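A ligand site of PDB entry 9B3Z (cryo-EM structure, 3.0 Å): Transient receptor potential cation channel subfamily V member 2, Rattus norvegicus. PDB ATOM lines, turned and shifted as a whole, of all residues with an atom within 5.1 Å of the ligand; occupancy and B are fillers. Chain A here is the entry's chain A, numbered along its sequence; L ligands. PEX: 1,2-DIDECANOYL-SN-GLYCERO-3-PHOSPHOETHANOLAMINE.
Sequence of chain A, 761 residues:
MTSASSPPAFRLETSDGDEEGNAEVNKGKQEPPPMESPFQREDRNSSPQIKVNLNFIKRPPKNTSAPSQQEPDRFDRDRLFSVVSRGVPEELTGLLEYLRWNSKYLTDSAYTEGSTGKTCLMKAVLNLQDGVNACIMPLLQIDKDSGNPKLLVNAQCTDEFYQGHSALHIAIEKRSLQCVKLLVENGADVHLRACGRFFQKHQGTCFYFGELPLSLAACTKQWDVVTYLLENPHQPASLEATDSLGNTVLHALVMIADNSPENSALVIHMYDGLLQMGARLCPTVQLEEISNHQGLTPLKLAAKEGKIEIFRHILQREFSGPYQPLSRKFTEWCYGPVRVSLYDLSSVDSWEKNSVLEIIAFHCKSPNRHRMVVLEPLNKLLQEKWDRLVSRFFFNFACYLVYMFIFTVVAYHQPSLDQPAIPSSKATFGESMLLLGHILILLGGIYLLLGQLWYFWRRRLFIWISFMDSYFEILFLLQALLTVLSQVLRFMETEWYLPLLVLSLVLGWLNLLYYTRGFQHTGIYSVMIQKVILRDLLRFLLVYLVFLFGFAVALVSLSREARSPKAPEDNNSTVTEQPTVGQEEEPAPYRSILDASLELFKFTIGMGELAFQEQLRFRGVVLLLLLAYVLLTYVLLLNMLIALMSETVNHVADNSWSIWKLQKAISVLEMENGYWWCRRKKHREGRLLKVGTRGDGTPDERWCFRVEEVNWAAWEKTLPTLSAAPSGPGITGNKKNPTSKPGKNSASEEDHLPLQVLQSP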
ATOM      1  N   PHE A 395      19.278  -6.267  14.149  1.00  0.00           N
ATOM      2  CA  PHE A 395      20.722  -6.258  14.366  1.00  0.00           C
ATOM      3  C   PHE A 395      21.412  -5.373  13.344  1.00  0.00           C
ATOM      4  O   PHE A 395      22.350  -4.632  13.675  1.00  0.00           O
ATOM      5  CB  PHE A 395      21.281  -7.673  14.310  1.00  0.00           C
ATOM      6  CG  PHE A 395      22.786  -7.733  14.421  1.00  0.00           C
ATOM      7  CD1 PHE A 395      23.410  -7.506  15.631  1.00  0.00           C
ATOM      8  CD2 PHE A 395      23.560  -8.011  13.307  1.00  0.00           C
ATOM      9  CE1 PHE A 395      24.794  -7.557  15.727  1.00  0.00           C
ATOM     10  CE2 PHE A 395      24.930  -8.063  13.403  1.00  0.00           C
ATOM     11  CZ  PHE A 395      25.554  -7.836  14.613  1.00  0.00           C
ATOM     12  N   ASN A 396      20.962  -5.421  12.088  1.00  0.00           N
ATOM     13  CA  ASN A 396      21.472  -4.498  11.079  1.00  0.00           C
ATOM     14  C   ASN A 396      21.115  -3.060  11.436  1.00  0.00           C
ATOM     15  O   ASN A 396      21.925  -2.144  11.252  1.00  0.00           O
ATOM     16  CB  ASN A 396      20.907  -4.867   9.704  1.00  0.00           C
ATOM     17  CG  ASN A 396      21.525  -6.135   9.147  1.00  0.00           C
ATOM     18  OD1 ASN A 396      22.333  -6.793   9.810  1.00  0.00           O
ATOM     19  ND2 ASN A 396      21.150  -6.484   7.924  1.00  0.00           N
ATOM     20  N   CYS A 399      23.392  -1.986  14.369  1.00  0.00           N
ATOM     21  CA  CYS A 399      24.752  -1.702  13.930  1.00  0.00           C
ATOM     22  C   CYS A 399      24.832  -0.370  13.204  1.00  0.00           C
ATOM     23  O   CYS A 399      25.860   0.315  13.255  1.00  0.00           O
ATOM     24  CB  CYS A 399      25.271  -2.833  13.054  1.00  0.00           C
ATOM     25  SG  CYS A 399      25.529  -4.389  13.914  1.00  0.00           S
ATOM     26  N   TYR A 400      23.757   0.024  12.523  1.00  0.00           N
ATOM     27  CA  TYR A 400      23.755   1.310  11.842  1.00  0.00           C
ATOM     28  C   TYR A 400      23.610   2.460  12.832  1.00  0.00           C
ATOM     29  O   TYR A 400      24.227   3.518  12.660  1.00  0.00           O
ATOM     30  CB  TYR A 400      22.639   1.356  10.799  1.00  0.00           C
ATOM     31  CG  TYR A 400      22.768   2.511   9.820  1.00  0.00           C
ATOM     32  CD1 TYR A 400      23.725   2.475   8.817  1.00  0.00           C
ATOM     33  CD2 TYR A 400      21.936   3.612   9.910  1.00  0.00           C
ATOM     34  CE1 TYR A 400      23.852   3.525   7.930  1.00  0.00           C
ATOM     35  CE2 TYR A 400      22.049   4.661   9.023  1.00  0.00           C
ATOM     36  CZ  TYR A 400      23.014   4.614   8.025  1.00  0.00           C
ATOM     37  OH  TYR A 400      23.134   5.654   7.144  1.00  0.00           O
ATOM     38  N   VAL A 402      24.670   2.424  15.949  1.00  0.00           N
ATOM     39  CA  VAL A 402      25.977   2.530  16.604  1.00  0.00           C
ATOM     40  C   VAL A 402      26.960   3.236  15.684  1.00  0.00           C
ATOM     41  O   VAL A 402      27.742   4.098  16.116  1.00  0.00           O
ATOM     42  CB  VAL A 402      26.490   1.139  17.014  1.00  0.00           C
ATOM     43  CG1 VAL A 402      27.957   1.202  17.405  1.00  0.00           C
ATOM     44  CG2 VAL A 402      25.651   0.595  18.161  1.00  0.00           C
ATOM     45  N   TYR A 403      26.946   2.889  14.396  1.00  0.00           N
ATOM     46  CA  TYR A 403      27.849   3.527  13.442  1.00  0.00           C
ATOM     47  C   TYR A 403      27.541   5.013  13.303  1.00  0.00           C
ATOM     48  O   TYR A 403      28.448   5.843  13.218  1.00  0.00           O
ATOM     49  CB  TYR A 403      27.743   2.826  12.084  1.00  0.00           C
ATOM     50  CG  TYR A 403      28.319   3.618  10.937  1.00  0.00           C
ATOM     51  CD1 TYR A 403      29.698   3.792  10.801  1.00  0.00           C
ATOM     52  CD2 TYR A 403      27.498   4.187   9.969  1.00  0.00           C
ATOM     53  CE1 TYR A 403      30.228   4.506   9.751  1.00  0.00           C
ATOM     54  CE2 TYR A 403      28.020   4.907   8.921  1.00  0.00           C
ATOM     55  CZ  TYR A 403      29.386   5.066   8.812  1.00  0.00           C
ATOM     56  OH  TYR A 403      29.916   5.780   7.761  1.00  0.00           O
ATOM     57  N   ILE A 406      28.611   6.937  16.498  1.00  0.00           N
ATOM     58  CA  ILE A 406      30.031   7.254  16.414  1.00  0.00           C
ATOM     59  C   ILE A 406      30.259   8.390  15.423  1.00  0.00           C
ATOM     60  O   ILE A 406      31.083   9.276  15.663  1.00  0.00           O
ATOM     61  CB  ILE A 406      30.838   5.996  16.028  1.00  0.00           C
ATOM     62  CG1 ILE A 406      30.786   4.972  17.163  1.00  0.00           C
ATOM     63  CG2 ILE A 406      32.278   6.353  15.704  1.00  0.00           C
ATOM     64  CD1 ILE A 406      31.142   3.566  16.745  1.00  0.00           C
ATOM     65  N   GLY A 444      33.770   1.539   8.726  1.00  0.00           N
ATOM     66  CA  GLY A 444      32.353   1.447   8.443  1.00  0.00           C
ATOM     67  C   GLY A 444      32.006   1.947   7.054  1.00  0.00           C
ATOM     68  O   GLY A 444      31.173   1.369   6.365  1.00  0.00           O
ATOM     69  N   TYR A 447      32.857  -0.677   4.629  1.00  0.00           N
ATOM     70  CA  TYR A 447      31.925  -1.796   4.744  1.00  0.00           C
ATOM     71  C   TYR A 447      30.645  -1.513   3.976  1.00  0.00           C
ATOM     72  O   TYR A 447      30.140  -2.365   3.237  1.00  0.00           O
ATOM     73  CB  TYR A 447      31.635  -2.078   6.218  1.00  0.00           C
ATOM     74  CG  TYR A 447      30.727  -3.267   6.454  1.00  0.00           C
ATOM     75  CD1 TYR A 447      29.345  -3.124   6.473  1.00  0.00           C
ATOM     76  CD2 TYR A 447      31.262  -4.528   6.649  1.00  0.00           C
ATOM     77  CE1 TYR A 447      28.523  -4.211   6.692  1.00  0.00           C
ATOM     78  CE2 TYR A 447      30.448  -5.621   6.864  1.00  0.00           C
ATOM     79  CZ  TYR A 447      29.078  -5.460   6.881  1.00  0.00           C
ATOM     80  OH  TYR A 447      28.256  -6.547   7.100  1.00  0.00           O
ATOM     81  N   LEU A 448      30.090  -0.305   4.138  1.00  0.00           N
ATOM     82  CA  LEU A 448      28.897   0.054   3.373  1.00  0.00           C
ATOM     83  C   LEU A 448      29.215   0.220   1.894  1.00  0.00           C
ATOM     84  O   LEU A 448      28.373  -0.067   1.030  1.00  0.00           O
ATOM     85  CB  LEU A 448      28.278   1.335   3.936  1.00  0.00           C
ATOM     86  CG  LEU A 448      27.324   1.186   5.125  1.00  0.00           C
ATOM     87  CD1 LEU A 448      28.036   1.472   6.431  1.00  0.00           C
ATOM     88  CD2 LEU A 448      26.129   2.103   4.958  1.00  0.00           C
ATOM     89  N   GLN A 452      27.288  -2.124  -0.788  1.00  0.00           N
ATOM     90  CA  GLN A 452      26.447  -1.572  -1.833  1.00  0.00           C
ATOM     91  C   GLN A 452      26.990  -1.871  -3.223  1.00  0.00           C
ATOM     92  O   GLN A 452      26.207  -2.059  -4.160  1.00  0.00           O
ATOM     93  CB  GLN A 452      26.292  -0.056  -1.644  1.00  0.00           C
ATOM     94  CG  GLN A 452      25.482   0.321  -0.421  1.00  0.00           C
ATOM     95  CD  GLN A 452      24.126  -0.345  -0.397  1.00  0.00           C
ATOM     96  OE1 GLN A 452      23.894  -1.269   0.390  1.00  0.00           O
ATOM     97  NE2 GLN A 452      23.227   0.100  -1.259  1.00  0.00           N
ATOM     98  N   PHE A 472      16.905   3.967  -1.579  1.00  0.00           N
ATOM     99  CA  PHE A 472      17.819   3.968  -0.438  1.00  0.00           C
ATOM    100  C   PHE A 472      19.119   3.233  -0.755  1.00  0.00           C
ATOM    101  O   PHE A 472      20.141   3.495  -0.112  1.00  0.00           O
ATOM    102  CB  PHE A 472      17.146   3.369   0.790  1.00  0.00           C
ATOM    103  CG  PHE A 472      16.277   4.332   1.531  1.00  0.00           C
ATOM    104  CD1 PHE A 472      16.843   5.327   2.309  1.00  0.00           C
ATOM    105  CD2 PHE A 472      14.901   4.251   1.444  1.00  0.00           C
ATOM    106  CE1 PHE A 472      16.049   6.216   2.988  1.00  0.00           C
ATOM    107  CE2 PHE A 472      14.106   5.153   2.129  1.00  0.00           C
ATOM    108  CZ  PHE A 472      14.680   6.129   2.898  1.00  0.00           C
ATOM    109  N   GLU A 473      19.095   2.310  -1.712  1.00  0.00           N
ATOM    110  CA  GLU A 473      20.328   1.631  -2.099  1.00  0.00           C
ATOM    111  C   GLU A 473      21.322   2.603  -2.733  1.00  0.00           C
ATOM    112  O   GLU A 473      22.534   2.451  -2.572  1.00  0.00           O
ATOM    113  CB  GLU A 473      20.020   0.482  -3.055  1.00  0.00           C
ATOM    114  CG  GLU A 473      18.791  -0.326  -2.669  1.00  0.00           C
ATOM    115  CD  GLU A 473      18.908  -0.997  -1.318  1.00  0.00           C
ATOM    116  OE1 GLU A 473      20.040  -1.261  -0.864  1.00  0.00           O
ATOM    117  OE2 GLU A 473      17.857  -1.262  -0.696  1.00  0.00           O
ATOM    118  N   PHE A 476      22.564   4.853   0.335  1.00  0.00           N
ATOM    119  CA  PHE A 476      23.523   4.140   1.168  1.00  0.00           C
ATOM    120  C   PHE A 476      24.879   4.032   0.501  1.00  0.00           C
ATOM    121  O   PHE A 476      25.901   3.927   1.188  1.00  0.00           O
ATOM    122  CB  PHE A 476      22.981   2.741   1.510  1.00  0.00           C
ATOM    123  CG  PHE A 476      22.189   2.701   2.785  1.00  0.00           C
ATOM    124  CD1 PHE A 476      20.881   3.136   2.820  1.00  0.00           C
ATOM    125  CD2 PHE A 476      22.751   2.201   3.955  1.00  0.00           C
ATOM    126  CE1 PHE A 476      20.147   3.091   3.990  1.00  0.00           C
ATOM    127  CE2 PHE A 476      22.023   2.163   5.127  1.00  0.00           C
ATOM    128  CZ  PHE A 476      20.714   2.607   5.145  1.00  0.00           C
ATOM    129  N   TYR A 514      15.057   3.905   6.002  1.00  0.00           N
ATOM    130  CA  TYR A 514      15.076   2.578   5.408  1.00  0.00           C
ATOM    131  C   TYR A 514      14.616   1.517   6.411  1.00  0.00           C
ATOM    132  O   TYR A 514      14.027   0.511   6.033  1.00  0.00           O
ATOM    133  CB  TYR A 514      16.474   2.231   4.897  1.00  0.00           C
ATOM    134  CG  TYR A 514      16.597   0.827   4.339  1.00  0.00           C
ATOM    135  CD1 TYR A 514      16.148   0.532   3.066  1.00  0.00           C
ATOM    136  CD2 TYR A 514      17.149  -0.194   5.099  1.00  0.00           C
ATOM    137  CE1 TYR A 514      16.249  -0.755   2.558  1.00  0.00           C
ATOM    138  CE2 TYR A 514      17.250  -1.473   4.607  1.00  0.00           C
ATOM    139  CZ  TYR A 514      16.800  -1.751   3.332  1.00  0.00           C
ATOM    140  OH  TYR A 514      16.900  -3.025   2.831  1.00  0.00           O
ATOM    141  N   TYR A 515      14.885   1.750   7.689  1.00  0.00           N
ATOM    142  CA  TYR A 515      14.539   0.795   8.733  1.00  0.00           C
ATOM    143  C   TYR A 515      13.161   1.038   9.325  1.00  0.00           C
ATOM    144  O   TYR A 515      12.773   0.329  10.261  1.00  0.00           O
ATOM    145  CB  TYR A 515      15.601   0.818   9.837  1.00  0.00           C
ATOM    146  CG  TYR A 515      17.001   0.546   9.320  1.00  0.00           C
ATOM    147  CD1 TYR A 515      17.807   1.572   8.866  1.00  0.00           C
ATOM    148  CD2 TYR A 515      17.497  -0.754   9.281  1.00  0.00           C
ATOM    149  CE1 TYR A 515      19.079   1.316   8.394  1.00  0.00           C
ATOM    150  CE2 TYR A 515      18.769  -1.010   8.809  1.00  0.00           C
ATOM    151  CZ  TYR A 515      19.560   0.027   8.362  1.00  0.00           C
ATOM    152  OH  TYR A 515      20.825  -0.223   7.893  1.00  0.00           O
ATOM    153  N   TYR A 675      25.513 -11.546   4.165  1.00  0.00           N
ATOM    154  CA  TYR A 675      26.403 -10.414   3.991  1.00  0.00           C
ATOM    155  C   TYR A 675      27.381 -10.672   2.848  1.00  0.00           C
ATOM    156  O   TYR A 675      27.600 -11.806   2.429  1.00  0.00           O
ATOM    157  CB  TYR A 675      27.156 -10.116   5.280  1.00  0.00           C
ATOM    158  CG  TYR A 675      26.264  -9.881   6.476  1.00  0.00           C
ATOM    159  CD1 TYR A 675      25.439  -8.777   6.545  1.00  0.00           C
ATOM    160  CD2 TYR A 675      26.248 -10.785   7.538  1.00  0.00           C
ATOM    161  CE1 TYR A 675      24.619  -8.559   7.629  1.00  0.00           C
ATOM    162  CE2 TYR A 675      25.421 -10.578   8.628  1.00  0.00           C
ATOM    163  CZ  TYR A 675      24.610  -9.459   8.670  1.00  0.00           C
ATOM    164  OH  TYR A 675      23.798  -9.251   9.760  1.00  0.00           O
ATOM    165  N   TRP A 677      30.576 -10.327   2.971  1.00  0.00           N
ATOM    166  CA  TRP A 677      31.741 -11.021   3.503  1.00  0.00           C
ATOM    167  C   TRP A 677      31.425 -12.434   3.991  1.00  0.00           C
ATOM    168  O   TRP A 677      32.355 -13.192   4.281  1.00  0.00           O
ATOM    169  CB  TRP A 677      32.351 -10.213   4.657  1.00  0.00           C
ATOM    170  CG  TRP A 677      31.369  -9.893   5.742  1.00  0.00           C
ATOM    171  CD1 TRP A 677      30.506  -8.842   5.784  1.00  0.00           C
ATOM    172  CD2 TRP A 677      31.171 -10.618   6.959  1.00  0.00           C
ATOM    173  NE1 TRP A 677      29.771  -8.882   6.945  1.00  0.00           N
ATOM    174  CE2 TRP A 677      30.164  -9.957   7.681  1.00  0.00           C
ATOM    175  CE3 TRP A 677      31.754 -11.771   7.503  1.00  0.00           C
ATOM    176  CZ2 TRP A 677      29.723 -10.407   8.925  1.00  0.00           C
ATOM    177  CZ3 TRP A 677      31.313 -12.217   8.738  1.00  0.00           C
ATOM    178  CH2 TRP A 677      30.304 -11.529   9.440  1.00  0.00           C
HETATM  179  O1  PEX L   1      20.753  -3.475   6.202  1.00  0.00           O
HETATM  180  O2  PEX L   1      22.849  -4.394   4.989  1.00  0.00           O
HETATM  181  P1  PEX L   1      22.110  -3.237   5.592  1.00  0.00           P
HETATM  182  O3  PEX L   1      23.055  -2.442   6.674  1.00  0.00           O
HETATM  183  C1  PEX L   1      23.474  -3.171   7.806  1.00  0.00           C
HETATM  184  C2  PEX L   1      24.950  -3.018   8.119  1.00  0.00           C
HETATM  185  C3  PEX L   1      25.374  -1.605   8.465  1.00  0.00           C
HETATM  186  O4  PEX L   1      26.767  -1.591   8.742  1.00  0.00           O
HETATM  187  C4  PEX L   1      27.270  -0.464   9.230  1.00  0.00           C
HETATM  188  O5  PEX L   1      26.621   0.541   9.356  1.00  0.00           O
HETATM  189  C5  PEX L   1      28.729  -0.607   9.570  1.00  0.00           C
HETATM  190  C6  PEX L   1      28.956  -1.221  10.948  1.00  0.00           C
HETATM  191  C7  PEX L   1      30.423  -1.155  11.363  1.00  0.00           C
HETATM  192  C8  PEX L   1      30.637  -1.568  12.813  1.00  0.00           C
HETATM  193  C9  PEX L   1      30.047  -0.577  13.810  1.00  0.00           C
HETATM  194  C10 PEX L   1      29.966  -1.128  15.229  1.00  0.00           C
HETATM  195  C11 PEX L   1      29.016  -2.311  15.356  1.00  0.00           C
HETATM  196  C12 PEX L   1      28.867  -2.817  16.788  1.00  0.00           C
HETATM  197  C13 PEX L   1      27.774  -3.866  16.932  1.00  0.00           C
HETATM  198  O6  PEX L   1      25.349  -3.866   9.201  1.00  0.00           O
HETATM  199  C14 PEX L   1      25.751  -5.109   8.934  1.00  0.00           C
HETATM  200  O7  PEX L   1      25.848  -5.549   7.820  1.00  0.00           O
HETATM  201  C15 PEX L   1      26.072  -5.862  10.192  1.00  0.00           C
HETATM  202  C16 PEX L   1      27.351  -5.415  10.879  1.00  0.00           C
HETATM  203  C17 PEX L   1      28.558  -6.246  10.458  1.00  0.00           C
HETATM  204  C18 PEX L   1      29.702  -6.167  11.465  1.00  0.00           C
HETATM  205  C19 PEX L   1      30.838  -7.132  11.155  1.00  0.00           C
HETATM  206  C20 PEX L   1      31.732  -6.677  10.016  1.00  0.00           C
HETATM  207  C21 PEX L   1      32.862  -7.650   9.703  1.00  0.00           C
HETATM  208  C22 PEX L   1      33.661  -7.273   8.458  1.00  0.00           C
HETATM  209  C23 PEX L   1      34.770  -8.253   8.142  1.00  0.00           C
HETATM  210  O8  PEX L   1      22.041  -1.978   4.560  1.00  0.00           O
HETATM  211  C24 PEX L   1      20.782  -1.724   3.957  1.00  0.00           C
HETATM  212  C25 PEX L   1      20.956  -0.945   2.678  1.00  0.00           C
HETATM  213  N1  PEX L   1      19.676  -0.676   2.027  1.00  0.00           N
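The side-chain hydroxyl (OH) of Tyr 447 is in hydrogen-bond range of an oxygen (O7) of the ligand (2.7 Å). OE1 of Glu 473 is in salt-bridge range of N1 of the ligand (3.0 Å). An oxygen (O3) of the ligand is in hydrogen-bond range of the side-chain hydroxyl (OH) of Tyr 515, at 3.4 Å. The side-chain amide nitrogen (ND2) of Asn 396 lies within hydrogen-bond range of an oxygen (O1) of the ligand (3.5 Å).
SG of Cys 399 touches C16 of the ligand (3.7 Å). CD1 of Tyr 400 touches O5 of the ligand, at 3.5 Å. CG1 of Val 402 touches C10 of the ligand, 3.8 Å away. Tyr 403 touches the ligand. CD1 of Leu 448 touches O5 of the ligand (3.4 Å). OE1 of Gln 452 touches C25 of the ligand, 3.7 Å away. Phe 476 touches the ligand (CD2 to C25, 3.8 Å). Tyr 514 touches the ligand (CZ to N1, 3.3 Å). CE1 of Tyr 675 touches O7 of the ligand (3.3 Å). Hydrophobic or aromatic side chains within 4 Å of the ligand: Tyr 400, Val 402, Tyr 403, Tyr 447, Leu 448, Phe 476, Tyr 514 and Tyr 675. 13 residues have an atom within 4 Å of the ligand: Asn 396, Cys 399, Tyr 400, Val 402, Tyr 403, Tyr 447, Leu 448, Gln 452, Glu 473, Phe 476, Tyr 514, Tyr 515 and Tyr 675. The nearest printed residue that does not touch the ligand is Phe 395 (4.1 Å).
OH of Tyr 447 lies within hydrogen-bond range of NE1 of Trp 677 (2.8 Å). O of Glu 473 is in hydrogen-bond range of NE2 of Gln 452 (2.8 Å). OH of Tyr 675 sits at hydrogen-bond distance from OD1 of Asn 396 (2.9 Å). The side-chain sulfur of Cys 399 lies within hydrogen-bond range of the backbone carbonyl oxygen of Phe 395 (3.2 Å).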
